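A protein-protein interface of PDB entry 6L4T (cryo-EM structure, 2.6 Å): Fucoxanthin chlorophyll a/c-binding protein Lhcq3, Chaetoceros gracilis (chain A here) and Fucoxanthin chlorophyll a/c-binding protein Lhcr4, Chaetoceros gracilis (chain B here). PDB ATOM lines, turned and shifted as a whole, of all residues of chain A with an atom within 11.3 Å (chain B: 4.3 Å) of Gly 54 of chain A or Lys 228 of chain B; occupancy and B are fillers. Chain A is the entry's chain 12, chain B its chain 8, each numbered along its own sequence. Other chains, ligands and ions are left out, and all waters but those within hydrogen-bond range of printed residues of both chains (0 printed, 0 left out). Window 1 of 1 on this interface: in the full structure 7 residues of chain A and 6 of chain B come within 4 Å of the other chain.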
ATOM      1  N   LEU A  32      -1.223  16.967  11.184  1.00  0.00           N
ATOM      2  CA  LEU A  32      -0.566  16.353  10.034  1.00  0.00           C
ATOM      3  C   LEU A  32      -0.276  17.382   8.950  1.00  0.00           C
ATOM      4  O   LEU A  32      -0.797  18.490   8.984  1.00  0.00           O
ATOM      5  CB  LEU A  32      -1.418  15.220   9.466  1.00  0.00           C
ATOM      6  CG  LEU A  32      -1.044  13.799   9.891  1.00  0.00           C
ATOM      7  CD1 LEU A  32      -1.423  13.527  11.340  1.00  0.00           C
ATOM      8  CD2 LEU A  32      -1.699  12.788   8.970  1.00  0.00           C
ATOM      9  N   ASP A  46       2.595  21.784  15.928  1.00  0.00           N
ATOM     10  CA  ASP A  46       2.000  21.155  17.096  1.00  0.00           C
ATOM     11  C   ASP A  46       3.075  20.841  18.127  1.00  0.00           C
ATOM     12  O   ASP A  46       3.434  19.670  18.292  1.00  0.00           O
ATOM     13  CB  ASP A  46       1.265  19.879  16.691  1.00  0.00           C
ATOM     14  CG  ASP A  46       0.120  19.544  17.613  1.00  0.00           C
ATOM     15  OD1 ASP A  46      -0.395  18.414  17.527  1.00  0.00           O
ATOM     16  OD2 ASP A  46      -0.265  20.407  18.421  1.00  0.00           O
ATOM     17  N   LEU A  48       2.956  21.063  21.481  1.00  0.00           N
ATOM     18  CA  LEU A  48       2.397  20.336  22.610  1.00  0.00           C
ATOM     19  C   LEU A  48       1.759  19.020  22.201  1.00  0.00           C
ATOM     20  O   LEU A  48       1.269  18.301  23.077  1.00  0.00           O
ATOM     21  CB  LEU A  48       1.367  21.192  23.346  1.00  0.00           C
ATOM     22  CG  LEU A  48       1.906  22.453  24.011  1.00  0.00           C
ATOM     23  CD1 LEU A  48       0.815  23.110  24.823  1.00  0.00           C
ATOM     24  CD2 LEU A  48       3.098  22.122  24.885  1.00  0.00           C
ATOM     25  N   ASN A  49       1.749  18.716  20.898  1.00  0.00           N
ATOM     26  CA  ASN A  49       1.284  17.447  20.332  1.00  0.00           C
ATOM     27  C   ASN A  49      -0.180  17.177  20.671  1.00  0.00           C
ATOM     28  O   ASN A  49      -0.558  16.083  21.085  1.00  0.00           O
ATOM     29  CB  ASN A  49       2.176  16.284  20.768  1.00  0.00           C
ATOM     30  CG  ASN A  49       2.231  15.185  19.742  1.00  0.00           C
ATOM     31  OD1 ASN A  49       2.531  15.427  18.576  1.00  0.00           O
ATOM     32  ND2 ASN A  49       1.926  13.966  20.164  1.00  0.00           N
ATOM     33  N   LEU A  50      -1.012  18.197  20.481  1.00  0.00           N
ATOM     34  CA  LEU A  50      -2.425  18.101  20.814  1.00  0.00           C
ATOM     35  C   LEU A  50      -3.233  17.310  19.796  1.00  0.00           C
ATOM     36  O   LEU A  50      -4.404  17.023  20.058  1.00  0.00           O
ATOM     37  CB  LEU A  50      -3.024  19.498  20.955  1.00  0.00           C
ATOM     38  CG  LEU A  50      -2.545  20.334  22.137  1.00  0.00           C
ATOM     39  CD1 LEU A  50      -3.157  21.714  22.088  1.00  0.00           C
ATOM     40  CD2 LEU A  50      -2.899  19.650  23.432  1.00  0.00           C
ATOM     41  N   ALA A  51      -2.658  16.971  18.642  1.00  0.00           N
ATOM     42  CA  ALA A  51      -3.400  16.217  17.640  1.00  0.00           C
ATOM     43  C   ALA A  51      -3.541  14.753  18.017  1.00  0.00           C
ATOM     44  O   ALA A  51      -4.541  14.121  17.660  1.00  0.00           O
ATOM     45  CB  ALA A  51      -2.727  16.348  16.275  1.00  0.00           C
ATOM     46  N   ASP A  52      -2.566  14.204  18.729  1.00  0.00           N
ATOM     47  CA  ASP A  52      -2.617  12.823  19.177  1.00  0.00           C
ATOM     48  C   ASP A  52      -3.257  12.670  20.547  1.00  0.00           C
ATOM     49  O   ASP A  52      -3.347  11.547  21.047  1.00  0.00           O
ATOM     50  CB  ASP A  52      -1.210  12.230  19.198  1.00  0.00           C
ATOM     51  CG  ASP A  52      -0.455  12.502  17.924  1.00  0.00           C
ATOM     52  OD1 ASP A  52      -0.785  11.876  16.897  1.00  0.00           O
ATOM     53  OD2 ASP A  52       0.462  13.344  17.942  1.00  0.00           O
ATOM     54  N   SER A  53      -3.710  13.766  21.157  1.00  0.00           N
ATOM     55  CA  SER A  53      -4.320  13.698  22.477  1.00  0.00           C
ATOM     56  C   SER A  53      -5.673  13.006  22.457  1.00  0.00           C
ATOM     57  O   SER A  53      -6.102  12.484  23.490  1.00  0.00           O
ATOM     58  CB  SER A  53      -4.463  15.102  23.058  1.00  0.00           C
ATOM     59  OG  SER A  53      -5.462  15.835  22.377  1.00  0.00           O
ATOM     60  N   GLY A  54      -6.345  12.985  21.315  1.00  0.00           N
ATOM     61  CA  GLY A  54      -7.573  12.249  21.135  1.00  0.00           C
ATOM     62  C   GLY A  54      -7.463  11.309  19.951  1.00  0.00           C
ATOM     63  O   GLY A  54      -6.388  10.826  19.606  1.00  0.00           O
ATOM     64  N   SER A  55      -8.601  11.060  19.327  1.00  0.00           N
ATOM     65  CA  SER A  55      -8.681  10.206  18.159  1.00  0.00           C
ATOM     66  C   SER A  55      -8.661  11.048  16.889  1.00  0.00           C
ATOM     67  O   SER A  55      -8.418  12.256  16.918  1.00  0.00           O
ATOM     68  CB  SER A  55      -9.932   9.339  18.246  1.00  0.00           C
ATOM     69  OG  SER A  55      -9.829   8.459  19.344  1.00  0.00           O
ATOM     70  N   GLU A  56      -8.915  10.401  15.753  1.00  0.00           N
ATOM     71  CA  GLU A  56      -9.078  11.130  14.504  1.00  0.00           C
ATOM     72  C   GLU A  56     -10.387  11.897  14.466  1.00  0.00           C
ATOM     73  O   GLU A  56     -10.510  12.850  13.692  1.00  0.00           O
ATOM     74  CB  GLU A  56      -9.000  10.170  13.319  1.00  0.00           C
ATOM     75  CG  GLU A  56      -7.645   9.509  13.163  1.00  0.00           C
ATOM     76  CD  GLU A  56      -6.553  10.488  12.781  1.00  0.00           C
ATOM     77  OE1 GLU A  56      -6.839  11.450  12.037  1.00  0.00           O
ATOM     78  OE2 GLU A  56      -5.405  10.296  13.232  1.00  0.00           O
ATOM     79  N   GLU A  57     -11.364  11.501  15.277  1.00  0.00           N
ATOM     80  CA  GLU A  57     -12.577  12.284  15.441  1.00  0.00           C
ATOM     81  C   GLU A  57     -12.385  13.454  16.392  1.00  0.00           C
ATOM     82  O   GLU A  57     -13.205  14.374  16.392  1.00  0.00           O
ATOM     83  CB  GLU A  57     -13.711  11.395  15.943  1.00  0.00           C
ATOM     84  CG  GLU A  57     -13.830  10.087  15.204  1.00  0.00           C
ATOM     85  CD  GLU A  57     -15.230   9.520  15.253  1.00  0.00           C
ATOM     86  OE1 GLU A  57     -15.990   9.886  16.173  1.00  0.00           O
ATOM     87  OE2 GLU A  57     -15.573   8.708  14.368  1.00  0.00           O
ATOM     88  N   THR A  58     -11.331  13.437  17.205  1.00  0.00           N
ATOM     89  CA  THR A  58     -11.010  14.597  18.026  1.00  0.00           C
ATOM     90  C   THR A  58     -10.260  15.643  17.219  1.00  0.00           C
ATOM     91  O   THR A  58     -10.455  16.846  17.420  1.00  0.00           O
ATOM     92  CB  THR A  58     -10.189  14.174  19.242  1.00  0.00           C
ATOM     93  OG1 THR A  58     -10.764  12.995  19.812  1.00  0.00           O
ATOM     94  CG2 THR A  58     -10.188  15.262  20.289  1.00  0.00           C
ATOM     95  N   LEU A  59      -9.395  15.203  16.304  1.00  0.00           N
ATOM     96  CA  LEU A  59      -8.701  16.147  15.438  1.00  0.00           C
ATOM     97  C   LEU A  59      -9.661  16.775  14.440  1.00  0.00           C
ATOM     98  O   LEU A  59      -9.548  17.965  14.132  1.00  0.00           O
ATOM     99  CB  LEU A  59      -7.549  15.449  14.722  1.00  0.00           C
ATOM    100  CG  LEU A  59      -6.728  16.302  13.757  1.00  0.00           C
ATOM    101  CD1 LEU A  59      -6.149  17.507  14.466  1.00  0.00           C
ATOM    102  CD2 LEU A  59      -5.638  15.475  13.122  1.00  0.00           C
ATOM    103  N   ALA A  60     -10.629  15.999  13.953  1.00  0.00           N
ATOM    104  CA  ALA A  60     -11.640  16.533  13.049  1.00  0.00           C
ATOM    105  C   ALA A  60     -12.532  17.552  13.740  1.00  0.00           C
ATOM    106  O   ALA A  60     -13.049  18.463  13.089  1.00  0.00           O
ATOM    107  CB  ALA A  60     -12.482  15.396  12.485  1.00  0.00           C
ATOM    108  N   TRP A  61     -12.727  17.411  15.049  1.00  0.00           N
ATOM    109  CA  TRP A  61     -13.400  18.455  15.809  1.00  0.00           C
ATOM    110  C   TRP A  61     -12.510  19.678  15.962  1.00  0.00           C
ATOM    111  O   TRP A  61     -13.000  20.811  15.931  1.00  0.00           O
ATOM    112  CB  TRP A  61     -13.807  17.925  17.180  1.00  0.00           C
ATOM    113  CG  TRP A  61     -14.406  18.967  18.054  1.00  0.00           C
ATOM    114  CD1 TRP A  61     -13.767  19.715  18.995  1.00  0.00           C
ATOM    115  CD2 TRP A  61     -15.770  19.380  18.071  1.00  0.00           C
ATOM    116  NE1 TRP A  61     -14.648  20.572  19.593  1.00  0.00           N
ATOM    117  CE2 TRP A  61     -15.887  20.386  19.043  1.00  0.00           C
ATOM    118  CE3 TRP A  61     -16.905  19.001  17.353  1.00  0.00           C
ATOM    119  CZ2 TRP A  61     -17.094  21.012  19.322  1.00  0.00           C
ATOM    120  CZ3 TRP A  61     -18.098  19.625  17.629  1.00  0.00           C
ATOM    121  CH2 TRP A  61     -18.185  20.619  18.602  1.00  0.00           C
ATOM    122  N   PHE A  62     -11.206  19.465  16.155  1.00  0.00           N
ATOM    123  CA  PHE A  62     -10.278  20.574  16.338  1.00  0.00           C
ATOM    124  C   PHE A  62     -10.133  21.396  15.071  1.00  0.00           C
ATOM    125  O   PHE A  62      -9.957  22.615  15.144  1.00  0.00           O
ATOM    126  CB  PHE A  62      -8.905  20.059  16.762  1.00  0.00           C
ATOM    127  CG  PHE A  62      -8.832  19.595  18.187  1.00  0.00           C
ATOM    128  CD1 PHE A  62      -9.832  19.897  19.092  1.00  0.00           C
ATOM    129  CD2 PHE A  62      -7.745  18.859  18.620  1.00  0.00           C
ATOM    130  CE1 PHE A  62      -9.748  19.465  20.399  1.00  0.00           C
ATOM    131  CE2 PHE A  62      -7.656  18.429  19.922  1.00  0.00           C
ATOM    132  CZ  PHE A  62      -8.657  18.732  20.813  1.00  0.00           C
ATOM    133  N   THR A 141     -16.854  15.396  12.159  1.00  0.00           N
ATOM    134  CA  THR A 141     -16.102  14.559  13.080  1.00  0.00           C
ATOM    135  C   THR A 141     -15.982  13.128  12.586  1.00  0.00           C
ATOM    136  O   THR A 141     -15.074  12.413  13.013  1.00  0.00           O
ATOM    137  CB  THR A 141     -16.751  14.566  14.461  1.00  0.00           C
ATOM    138  OG1 THR A 141     -18.169  14.431  14.322  1.00  0.00           O
ATOM    139  CG2 THR A 141     -16.445  15.855  15.183  1.00  0.00           C
ATOM    140  N   PHE B 224     -11.915  11.298  22.956  1.00  0.00           N
ATOM    141  CA  PHE B 224     -10.488  11.229  23.247  1.00  0.00           C
ATOM    142  C   PHE B 224     -10.011   9.791  23.397  1.00  0.00           C
ATOM    143  O   PHE B 224      -8.844   9.498  23.125  1.00  0.00           O
ATOM    144  CB  PHE B 224     -10.162  11.995  24.525  1.00  0.00           C
ATOM    145  CG  PHE B 224     -10.194  13.484  24.377  1.00  0.00           C
ATOM    146  CD1 PHE B 224      -9.089  14.169  23.910  1.00  0.00           C
ATOM    147  CD2 PHE B 224     -11.320  14.201  24.738  1.00  0.00           C
ATOM    148  CE1 PHE B 224      -9.113  15.541  23.786  1.00  0.00           C
ATOM    149  CE2 PHE B 224     -11.350  15.573  24.615  1.00  0.00           C
ATOM    150  CZ  PHE B 224     -10.246  16.242  24.141  1.00  0.00           C
ATOM    151  N   LEU B 225     -10.885   8.891  23.839  1.00  0.00           N
ATOM    152  CA  LEU B 225     -10.518   7.515  24.137  1.00  0.00           C
ATOM    153  C   LEU B 225     -11.153   6.525  23.170  1.00  0.00           C
ATOM    154  O   LEU B 225     -11.460   5.394  23.550  1.00  0.00           O
ATOM    155  CB  LEU B 225     -10.906   7.160  25.572  1.00  0.00           C
ATOM    156  CG  LEU B 225     -10.129   7.806  26.715  1.00  0.00           C
ATOM    157  CD1 LEU B 225     -10.507   7.143  28.015  1.00  0.00           C
ATOM    158  CD2 LEU B 225      -8.635   7.710  26.480  1.00  0.00           C
ATOM    159  N   LYS B 226     -11.348   6.929  21.915  1.00  0.00           N
ATOM    160  CA  LYS B 226     -12.105   6.095  20.990  1.00  0.00           C
ATOM    161  C   LYS B 226     -11.263   4.945  20.450  1.00  0.00           C
ATOM    162  O   LYS B 226     -11.693   3.787  20.478  1.00  0.00           O
ATOM    163  CB  LYS B 226     -12.654   6.945  19.848  1.00  0.00           C
ATOM    164  CG  LYS B 226     -13.506   6.180  18.871  1.00  0.00           C
ATOM    165  CD  LYS B 226     -14.131   7.103  17.852  1.00  0.00           C
ATOM    166  CE  LYS B 226     -14.947   6.316  16.851  1.00  0.00           C
ATOM    167  NZ  LYS B 226     -16.090   5.625  17.508  1.00  0.00           N
ATOM    168  N   GLY B 227     -10.066   5.237  19.952  1.00  0.00           N
ATOM    169  CA  GLY B 227      -9.187   4.201  19.453  1.00  0.00           C
ATOM    170  C   GLY B 227      -8.018   3.871  20.347  1.00  0.00           C
ATOM    171  O   GLY B 227      -7.098   3.172  19.903  1.00  0.00           O
ATOM    172  N   LYS B 228      -8.015   4.332  21.592  1.00  0.00           N
ATOM    173  CA  LYS B 228      -6.850   4.208  22.444  1.00  0.00           C
ATOM    174  C   LYS B 228      -6.764   2.812  23.048  1.00  0.00           C
ATOM    175  O   LYS B 228      -7.757   2.091  23.160  1.00  0.00           O
ATOM    176  CB  LYS B 228      -6.888   5.260  23.547  1.00  0.00           C
ATOM    177  CG  LYS B 228      -7.042   6.675  23.042  1.00  0.00           C
ATOM    178  CD  LYS B 228      -5.931   7.050  22.091  1.00  0.00           C
ATOM    179  CE  LYS B 228      -5.854   8.550  21.915  1.00  0.00           C
ATOM    180  NZ  LYS B 228      -4.670   9.133  22.593  1.00  0.00           N
ATOM    181  N   SER B 229      -5.551   2.439  23.440  1.00  0.00           N
ATOM    182  CA  SER B 229      -5.313   1.129  24.019  1.00  0.00           C
ATOM    183  C   SER B 229      -5.795   1.086  25.463  1.00  0.00           C
ATOM    184  O   SER B 229      -6.175   2.097  26.053  1.00  0.00           O
ATOM    185  CB  SER B 229      -3.830   0.773  23.949  1.00  0.00           C
ATOM    186  OG  SER B 229      -3.079   1.540  24.869  1.00  0.00           O
ATOM    187  N   GLU B 230      -5.762  -0.115  26.041  1.00  0.00           N
ATOM    188  CA  GLU B 230      -6.211  -0.304  27.414  1.00  0.00           C
ATOM    189  C   GLU B 230      -5.240   0.286  28.425  1.00  0.00           C
ATOM    190  O   GLU B 230      -5.627   0.534  29.571  1.00  0.00           O
ATOM    191  CB  GLU B 230      -6.417  -1.796  27.686  1.00  0.00           C
ATOM    192  CG  GLU B 230      -7.365  -2.128  28.832  1.00  0.00           C
ATOM    193  CD  GLU B 230      -8.658  -1.334  28.788  1.00  0.00           C
ATOM    194  OE1 GLU B 230      -9.010  -0.716  29.816  1.00  0.00           O
ATOM    195  OE2 GLU B 230      -9.333  -1.340  27.737  1.00  0.00           O
ATOM    196  N   GLU B 232      -3.351   3.272  27.948  1.00  0.00           N
ATOM    197  CA  GLU B 232      -3.480   4.721  27.992  1.00  0.00           C
ATOM    198  C   GLU B 232      -4.890   5.167  28.340  1.00  0.00           C
ATOM    199  O   GLU B 232      -5.082   6.330  28.706  1.00  0.00           O
ATOM    200  CB  GLU B 232      -3.052   5.335  26.663  1.00  0.00           C
ATOM    201  CG  GLU B 232      -3.773   4.782  25.463  1.00  0.00           C
ATOM    202  CD  GLU B 232      -2.973   4.941  24.187  1.00  0.00           C
ATOM    203  OE1 GLU B 232      -1.763   5.231  24.279  1.00  0.00           O
ATOM    204  OE2 GLU B 232      -3.554   4.784  23.092  1.00  0.00           O
ATOM    205  N   ILE B 233      -5.875   4.278  28.222  1.00  0.00           N
ATOM    206  CA  ILE B 233      -7.181   4.549  28.805  1.00  0.00           C
ATOM    207  C   ILE B 233      -7.077   4.548  30.323  1.00  0.00           C
ATOM    208  O   ILE B 233      -7.652   5.410  31.000  1.00  0.00           O
ATOM    209  CB  ILE B 233      -8.210   3.528  28.282  1.00  0.00           C
ATOM    210  CG1 ILE B 233      -8.743   3.967  26.921  1.00  0.00           C
ATOM    211  CG2 ILE B 233      -9.377   3.335  29.240  1.00  0.00           C
ATOM    212  CD1 ILE B 233      -9.632   2.953  26.269  1.00  0.00           C
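OG of Ser 55 of chain A lies close to N of Lys 226 of chain B (3.4 Å).
The backbone NH of Gly 227 of chain B is in hydrogen-bond range of the side-chain hydroxyl of Ser 55 of chain A (3.3 Å).
O of Asp 52 of chain A sits at hydrogen-bond distance from NZ of Lys 228 of chain B, at 3.2 Å.
The side-chain amide nitrogen (ND2) of Asn 49 of chain A lies within hydrogen-bond range of the side-chain carboxylate (OD2) of Asp 52 of chain A, at 2.7 Å.
O of Leu 50 of chain A sits at hydrogen-bond distance from OG of Ser 53 of chain A (2.8 Å).
N of Ser 55 of chain A lies within hydrogen-bond range of OG1 of Thr 58 of chain A.
Among the printed residues, merely in contact across the chains: Ser 53 of chain A with Phe 224 of chain B, Ser 53 of chain A with Lys 228 of chain B, Gly 54 of chain A with Phe 224 of chain B, Gly 54 of chain A with Lys 228 of chain B, Glu 57 of chain A with Lys 226 of chain B and Thr 58 of chain A with Phe 224 of chain B.
Of the printed residues of chain B, Asp 52 of chain A touches Lys 228.
Of the printed residues of chain B, Ser 53 of chain A touches Phe 224 (3.5 Å) and Lys 228 (3.8 Å).
Printed residues of chain B within 4 Å of Glu 57 of chain A: Lys 226.
Printed residues of chain B within 4 Å of Thr 58 of chain A: Phe 224.
No residue of chain A comes within 4 Å of Leu 225 of chain B.
Of the printed residues of chain A, Lys 228 of chain B touches Asp 52, Ser 53 and Gly 54.
No residue of chain A comes within 4 Å of Ser 229 of chain B.
No residue of chain A comes within 4 Å of Glu 232 of chain B.
The nearest printed residue of chain B that does not touch Gly 54 of chain A is Leu 225 of chain B (5.4 Å).
The nearest printed residue of chain B that does not touch Glu 57 of chain A is Phe 224 of chain B (6.9 Å).
Printed residues of chain A that touch a printed residue of chain B: Asp 52, Ser 53, Gly 54, Ser 55, Glu 57 and Thr 58.
Hydrophobic or aromatic side chains of chain B within 4 Å of the printed part of chain A: Phe 224.
Among the printed residues, no Asp or Glu carboxylate lies within 4 Å of a Lys or Arg side-chain nitrogen of the other chain.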
